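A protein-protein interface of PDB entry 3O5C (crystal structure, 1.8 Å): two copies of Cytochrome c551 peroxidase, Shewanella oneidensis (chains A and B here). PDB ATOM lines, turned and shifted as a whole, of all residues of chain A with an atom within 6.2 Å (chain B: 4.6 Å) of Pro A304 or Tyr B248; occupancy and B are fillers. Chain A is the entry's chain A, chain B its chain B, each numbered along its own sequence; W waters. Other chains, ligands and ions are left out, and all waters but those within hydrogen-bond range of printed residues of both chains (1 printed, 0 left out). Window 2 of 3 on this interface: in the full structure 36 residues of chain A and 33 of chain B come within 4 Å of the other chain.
NH1 of Arg A38 sits at hydrogen-bond distance from OH of Tyr B248 (3.5 Å). N of Ser A305 sits at hydrogen-bond distance from OH of Tyr B248, 2.8 Å away.
The guanidinium group (NH1) of Arg A38 lies within hydrogen-bond range of the side-chain sulfur (SD) of Met A125. NH1 of Arg A38 is in hydrogen-bond range of OG of Ser A305. The backbone carbonyl oxygen (O) of Asn A306 sits at hydrogen-bond distance from the guanidinium group (NH2) of Arg A311, at 3.2 Å. O of Pro A303 is in hydrogen-bond range of NH1 of Arg A38 (2.9 Å).
No position is printed for both chains. Of the 6 pairs that touch across the chains among the printed residues, none has its exchanged pair printed and touching as well.
Water W1 bridges O of Ser A305 (3.4 Å) and O of Trp B257 (3.5 Å).
CG of Pro A304 touches OE2 of Glu B245, at 3.9 Å. Leu B246 touches Pro A304 (CD2 to CB, 3.9 Å). Tyr B248 touches Pro A304 (OH to CA, 3.6 Å). CB of Trp B257 touches NH1 of Arg A311 (3.7 Å).
Of the printed residues of chain B, Pro A304 touches Glu B245 (3.9 Å), Leu B246 (3.9 Å) and Tyr B248 (3.6 Å). Tyr B248 touches just these residues of chain A: Arg A38 (3.5 Å), Pro A304 (3.6 Å) and Ser A305 (2.8 Å). Of the printed residues of chain B, Ser A305 touches Tyr B248. Printed residues of chain B within 4 Å of Arg A38: Tyr B248 (3.5 Å). Of the printed residues of chain A, Glu B245 touches Pro A304. Printed residues of chain A within 4 Å of Leu B246: Pro A304. Asn A306 touches none of the printed residues of chain B. The nearest printed residue of chain B that does not touch Pro A304 is Thr B247 (6.7 Å). The nearest printed residue of chain B that does not touch Ser A305 is Glu B245 (5.2 Å).
Printed residues of chain B that touch a printed residue of chain A: Glu B245, Leu B246, Tyr B248 and Trp B257. Of the 11 printed residues of chain A, 4 touch a printed residue of chain B. Hydrophobic or aromatic side chains of chain A that line the printed part of chain B: Pro A304. Along chain A the printed residues that touch a printed residue of chain B span positions 38 to 311. Among the printed residues, 6 pairs touch across the chains. Among the printed residues, no Asp or Glu carboxylate lies within 4 Å of a Lys or Arg side-chain nitrogen of the other chain.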
ATOM      1  N   ARG A  38      18.732  -1.880   7.785  1.00  0.00           N
ATOM      2  CA  ARG A  38      17.353  -1.820   8.258  1.00  0.00           C
ATOM      3  C   ARG A  38      16.495  -0.824   7.445  1.00  0.00           C
ATOM      4  O   ARG A  38      15.306  -0.700   7.692  1.00  0.00           O
ATOM      5  CB  ARG A  38      17.310  -1.562   9.761  1.00  0.00           C
ATOM      6  CG  ARG A  38      17.873  -2.737  10.568  1.00  0.00           C
ATOM      7  CD  ARG A  38      18.185  -2.363  12.009  1.00  0.00           C
ATOM      8  NE  ARG A  38      19.216  -1.349  12.071  1.00  0.00           N
ATOM      9  CZ  ARG A  38      19.741  -0.837  13.178  1.00  0.00           C
ATOM     10  NH1 ARG A  38      19.336  -1.232  14.382  1.00  0.00           N
ATOM     11  NH2 ARG A  38      20.690   0.099  13.069  1.00  0.00           N
ATOM     12  N   MET A 125      14.897   4.600  16.920  1.00  0.00           N
ATOM     13  CA  MET A 125      16.161   4.534  17.666  1.00  0.00           C
ATOM     14  C   MET A 125      16.615   5.912  18.147  1.00  0.00           C
ATOM     15  O   MET A 125      16.894   6.778  17.338  1.00  0.00           O
ATOM     16  CB  MET A 125      17.232   3.868  16.812  1.00  0.00           C
ATOM     17  CG  MET A 125      16.891   2.406  16.512  1.00  0.00           C
ATOM     18  SD  MET A 125      18.039   1.596  15.392  1.00  0.00           S
ATOM     19  CE  MET A 125      17.239   1.804  13.804  1.00  0.00           C
ATOM     20  N   PRO A 126      16.678   6.117  19.471  1.00  0.00           N
ATOM     21  CA  PRO A 126      17.096   7.409  20.047  1.00  0.00           C
ATOM     22  C   PRO A 126      18.408   7.973  19.477  1.00  0.00           C
ATOM     23  O   PRO A 126      18.517   9.190  19.267  1.00  0.00           O
ATOM     24  CB  PRO A 126      17.262   7.099  21.530  1.00  0.00           C
ATOM     25  CG  PRO A 126      16.414   5.928  21.790  1.00  0.00           C
ATOM     26  CD  PRO A 126      16.250   5.166  20.511  1.00  0.00           C
ATOM     27  N   ALA A 127      19.388   7.101  19.234  1.00  0.00           N
ATOM     28  CA  ALA A 127      20.672   7.532  18.675  1.00  0.00           C
ATOM     29  C   ALA A 127      20.487   8.192  17.301  1.00  0.00           C
ATOM     30  O   ALA A 127      21.114   9.200  17.014  1.00  0.00           O
ATOM     31  CB  ALA A 127      21.652   6.352  18.589  1.00  0.00           C
ATOM     32  N   LEU A 302      26.201   1.403  13.967  1.00  0.00           N
ATOM     33  CA  LEU A 302      24.786   1.710  13.934  1.00  0.00           C
ATOM     34  C   LEU A 302      24.169   1.368  15.272  1.00  0.00           C
ATOM     35  O   LEU A 302      24.607   0.422  15.938  1.00  0.00           O
ATOM     36  CB  LEU A 302      24.098   0.915  12.820  1.00  0.00           C
ATOM     37  CG  LEU A 302      24.693   1.133  11.439  1.00  0.00           C
ATOM     38  CD1 LEU A 302      23.966   0.309  10.342  1.00  0.00           C
ATOM     39  CD2 LEU A 302      24.659   2.610  11.153  1.00  0.00           C
ATOM     40  N   PRO A 303      23.138   2.133  15.676  1.00  0.00           N
ATOM     41  CA  PRO A 303      22.525   1.862  16.953  1.00  0.00           C
ATOM     42  C   PRO A 303      21.742   0.565  16.947  1.00  0.00           C
ATOM     43  O   PRO A 303      21.380   0.081  15.877  1.00  0.00           O
ATOM     44  CB  PRO A 303      21.597   3.070  17.168  1.00  0.00           C
ATOM     45  CG  PRO A 303      21.369   3.625  15.884  1.00  0.00           C
ATOM     46  CD  PRO A 303      22.520   3.292  15.008  1.00  0.00           C
ATOM     47  N   PRO A 304      21.508  -0.015  18.138  1.00  0.00           N
ATOM     48  CA  PRO A 304      20.699  -1.219  18.252  1.00  0.00           C
ATOM     49  C   PRO A 304      19.207  -0.951  18.047  1.00  0.00           C
ATOM     50  O   PRO A 304      18.690   0.084  18.488  1.00  0.00           O
ATOM     51  CB  PRO A 304      20.927  -1.653  19.703  1.00  0.00           C
ATOM     52  CG  PRO A 304      21.256  -0.363  20.431  1.00  0.00           C
ATOM     53  CD  PRO A 304      22.046   0.423  19.437  1.00  0.00           C
ATOM     54  N   SER A 305      18.526  -1.886  17.395  1.00  0.00           N
ATOM     55  CA  SER A 305      17.075  -1.885  17.358  1.00  0.00           C
ATOM     56  C   SER A 305      16.559  -2.005  18.772  1.00  0.00           C
ATOM     57  O   SER A 305      17.242  -2.500  19.654  1.00  0.00           O
ATOM     58  CB  SER A 305      16.548  -3.069  16.557  1.00  0.00           C
ATOM     59  OG  SER A 305      16.961  -2.968  15.214  1.00  0.00           O
ATOM     60  N   ASN A 306      15.332  -1.570  18.965  1.00  0.00           N
ATOM     61  CA  ASN A 306      14.684  -1.682  20.247  1.00  0.00           C
ATOM     62  C   ASN A 306      13.252  -2.163  20.022  1.00  0.00           C
ATOM     63  O   ASN A 306      12.906  -2.613  18.926  1.00  0.00           O
ATOM     64  CB  ASN A 306      14.790  -0.345  20.976  1.00  0.00           C
ATOM     65  CG  ASN A 306      14.116   0.782  20.232  1.00  0.00           C
ATOM     66  OD1 ASN A 306      12.964   0.664  19.821  1.00  0.00           O
ATOM     67  ND2 ASN A 306      14.814   1.890  20.082  1.00  0.00           N
ATOM     68  N   THR A 309      11.287  -0.756  17.048  1.00  0.00           N
ATOM     69  CA  THR A 309      11.865  -0.888  15.716  1.00  0.00           C
ATOM     70  C   THR A 309      11.177  -2.045  15.005  1.00  0.00           C
ATOM     71  O   THR A 309      11.194  -3.177  15.512  1.00  0.00           O
ATOM     72  CB  THR A 309      13.363  -1.164  15.787  1.00  0.00           C
ATOM     73  OG1 THR A 309      13.973  -0.232  16.692  1.00  0.00           O
ATOM     74  CG2 THR A 309      14.006  -1.058  14.398  1.00  0.00           C
ATOM     75  N   ARG A 311      10.726  -5.207  13.026  1.00  0.00           N
ATOM     76  CA  ARG A 311      11.665  -6.314  12.811  1.00  0.00           C
ATOM     77  C   ARG A 311      11.934  -6.480  11.313  1.00  0.00           C
ATOM     78  O   ARG A 311      11.094  -6.123  10.485  1.00  0.00           O
ATOM     79  CB  ARG A 311      11.125  -7.633  13.382  1.00  0.00           C
ATOM     80  CG  ARG A 311      10.655  -7.610  14.833  1.00  0.00           C
ATOM     81  CD  ARG A 311      11.634  -6.905  15.734  1.00  0.00           C
ATOM     82  NE  ARG A 311      11.263  -6.957  17.148  1.00  0.00           N
ATOM     83  CZ  ARG A 311      11.957  -6.359  18.113  1.00  0.00           C
ATOM     84  NH1 ARG A 311      11.553  -6.455  19.377  1.00  0.00           N
ATOM     85  NH2 ARG A 311      13.060  -5.662  17.821  1.00  0.00           N
ATOM     86  N   ALA B  60      21.758  -9.990  12.668  1.00  0.00           N
ATOM     87  CA  ALA B  60      20.620  -9.623  13.513  1.00  0.00           C
ATOM     88  C   ALA B  60      19.279 -10.158  12.975  1.00  0.00           C
ATOM     89  O   ALA B  60      18.216  -9.526  13.120  1.00  0.00           O
ATOM     90  CB  ALA B  60      20.575  -8.116  13.733  1.00  0.00           C
ATOM     91  N   LEU B  61      19.354 -11.328  12.356  1.00  0.00           N
ATOM     92  CA  LEU B  61      18.207 -12.004  11.779  1.00  0.00           C
ATOM     93  C   LEU B  61      18.018 -13.297  12.534  1.00  0.00           C
ATOM     94  O   LEU B  61      18.927 -13.742  13.234  1.00  0.00           O
ATOM     95  CB  LEU B  61      18.456 -12.337  10.305  1.00  0.00           C
ATOM     96  CG  LEU B  61      18.813 -11.150   9.440  1.00  0.00           C
ATOM     97  CD1 LEU B  61      19.230 -11.613   8.060  1.00  0.00           C
ATOM     98  CD2 LEU B  61      17.652 -10.161   9.382  1.00  0.00           C
ATOM     99  N   ILE B 244      25.648  -8.237  24.152  1.00  0.00           N
ATOM    100  CA  ILE B 244      24.388  -8.946  23.970  1.00  0.00           C
ATOM    101  C   ILE B 244      23.254  -7.978  23.582  1.00  0.00           C
ATOM    102  O   ILE B 244      22.328  -8.354  22.865  1.00  0.00           O
ATOM    103  CB  ILE B 244      24.002  -9.788  25.224  1.00  0.00           C
ATOM    104  CG1 ILE B 244      22.960 -10.852  24.858  1.00  0.00           C
ATOM    105  CG2 ILE B 244      23.562  -8.885  26.384  1.00  0.00           C
ATOM    106  CD1 ILE B 244      23.445 -11.832  23.752  1.00  0.00           C
ATOM    107  N   GLU B 245      23.345  -6.735  24.037  1.00  0.00           N
ATOM    108  CA  GLU B 245      22.391  -5.679  23.655  1.00  0.00           C
ATOM    109  C   GLU B 245      22.227  -5.544  22.142  1.00  0.00           C
ATOM    110  O   GLU B 245      21.134  -5.208  21.681  1.00  0.00           O
ATOM    111  CB  GLU B 245      22.852  -4.333  24.209  1.00  0.00           C
ATOM    112  CG  GLU B 245      22.105  -3.102  23.666  1.00  0.00           C
ATOM    113  CD  GLU B 245      22.706  -1.788  24.141  1.00  0.00           C
ATOM    114  OE1 GLU B 245      23.916  -1.754  24.429  1.00  0.00           O
ATOM    115  OE2 GLU B 245      21.975  -0.773  24.202  1.00  0.00           O
ATOM    116  N   LEU B 246      23.315  -5.783  21.402  1.00  0.00           N
ATOM    117  CA  LEU B 246      23.383  -5.592  19.950  1.00  0.00           C
ATOM    118  C   LEU B 246      23.120  -6.826  19.092  1.00  0.00           C
ATOM    119  O   LEU B 246      23.020  -6.709  17.872  1.00  0.00           O
ATOM    120  CB  LEU B 246      24.776  -5.083  19.551  1.00  0.00           C
ATOM    121  CG  LEU B 246      25.459  -4.051  20.442  1.00  0.00           C
ATOM    122  CD1 LEU B 246      26.830  -3.673  19.863  1.00  0.00           C
ATOM    123  CD2 LEU B 246      24.574  -2.840  20.594  1.00  0.00           C
ATOM    124  N   THR B 247      23.053  -8.006  19.705  1.00  0.00           N
ATOM    125  CA  THR B 247      23.130  -9.259  18.951  1.00  0.00           C
ATOM    126  C   THR B 247      21.813 -10.050  18.915  1.00  0.00           C
ATOM    127  O   THR B 247      21.810 -11.259  18.679  1.00  0.00           O
ATOM    128  CB  THR B 247      24.299 -10.130  19.465  1.00  0.00           C
ATOM    129  OG1 THR B 247      24.139 -10.400  20.867  1.00  0.00           O
ATOM    130  CG2 THR B 247      25.618  -9.397  19.239  1.00  0.00           C
ATOM    131  N   TYR B 248      20.705  -9.347  19.138  1.00  0.00           N
ATOM    132  CA  TYR B 248      19.343  -9.863  18.896  1.00  0.00           C
ATOM    133  C   TYR B 248      19.181 -10.417  17.464  1.00  0.00           C
ATOM    134  O   TYR B 248      19.932 -10.038  16.560  1.00  0.00           O
ATOM    135  CB  TYR B 248      18.301  -8.751  19.128  1.00  0.00           C
ATOM    136  CG  TYR B 248      18.678  -7.480  18.399  1.00  0.00           C
ATOM    137  CD1 TYR B 248      19.312  -6.429  19.066  1.00  0.00           C
ATOM    138  CD2 TYR B 248      18.475  -7.363  17.029  1.00  0.00           C
ATOM    139  CE1 TYR B 248      19.694  -5.279  18.385  1.00  0.00           C
ATOM    140  CE2 TYR B 248      18.846  -6.239  16.355  1.00  0.00           C
ATOM    141  CZ  TYR B 248      19.466  -5.199  17.031  1.00  0.00           C
ATOM    142  OH  TYR B 248      19.838  -4.083  16.322  1.00  0.00           O
ATOM    143  N   PRO B 249      18.234 -11.354  17.266  1.00  0.00           N
ATOM    144  CA  PRO B 249      17.490 -12.065  18.316  1.00  0.00           C
ATOM    145  C   PRO B 249      18.351 -13.119  19.033  1.00  0.00           C
ATOM    146  O   PRO B 249      19.489 -13.353  18.660  1.00  0.00           O
ATOM    147  CB  PRO B 249      16.345 -12.729  17.552  1.00  0.00           C
ATOM    148  CG  PRO B 249      16.754 -12.795  16.155  1.00  0.00           C
ATOM    149  CD  PRO B 249      17.890 -11.843  15.922  1.00  0.00           C
ATOM    150  N   TYR B 250      17.794 -13.793  20.034  1.00  0.00           N
ATOM    151  CA  TYR B 250      18.626 -14.572  20.947  1.00  0.00           C
ATOM    152  C   TYR B 250      18.392 -16.064  20.893  1.00  0.00           C
ATOM    153  O   TYR B 250      17.372 -16.543  20.375  1.00  0.00           O
ATOM    154  CB  TYR B 250      18.482 -14.052  22.380  1.00  0.00           C
ATOM    155  CG  TYR B 250      18.801 -12.586  22.483  1.00  0.00           C
ATOM    156  CD1 TYR B 250      20.112 -12.136  22.317  1.00  0.00           C
ATOM    157  CD2 TYR B 250      17.804 -11.640  22.705  1.00  0.00           C
ATOM    158  CE1 TYR B 250      20.417 -10.799  22.384  1.00  0.00           C
ATOM    159  CE2 TYR B 250      18.106 -10.295  22.780  1.00  0.00           C
ATOM    160  CZ  TYR B 250      19.415  -9.884  22.608  1.00  0.00           C
ATOM    161  OH  TYR B 250      19.725  -8.554  22.661  1.00  0.00           O
ATOM    162  N   TRP B 257      13.290 -11.954  20.519  1.00  0.00           N
ATOM    163  CA  TRP B 257      13.762 -10.649  20.068  1.00  0.00           C
ATOM    164  C   TRP B 257      14.196  -9.721  21.189  1.00  0.00           C
ATOM    165  O   TRP B 257      15.080  -8.885  20.976  1.00  0.00           O
ATOM    166  CB  TRP B 257      12.715  -9.963  19.188  1.00  0.00           C
ATOM    167  CG  TRP B 257      12.731 -10.518  17.810  1.00  0.00           C
ATOM    168  CD1 TRP B 257      11.936 -11.498  17.314  1.00  0.00           C
ATOM    169  CD2 TRP B 257      13.620 -10.144  16.758  1.00  0.00           C
ATOM    170  NE1 TRP B 257      12.272 -11.764  16.011  1.00  0.00           N
ATOM    171  CE2 TRP B 257      13.312 -10.954  15.648  1.00  0.00           C
ATOM    172  CE3 TRP B 257      14.656  -9.214  16.649  1.00  0.00           C
ATOM    173  CZ2 TRP B 257      13.992 -10.855  14.437  1.00  0.00           C
ATOM    174  CZ3 TRP B 257      15.322  -9.106  15.438  1.00  0.00           C
ATOM    175  CH2 TRP B 257      14.990  -9.926  14.352  1.00  0.00           C
HETATM  176  O   HOH W   1      15.908  -5.595  20.136  1.00  0.00           O
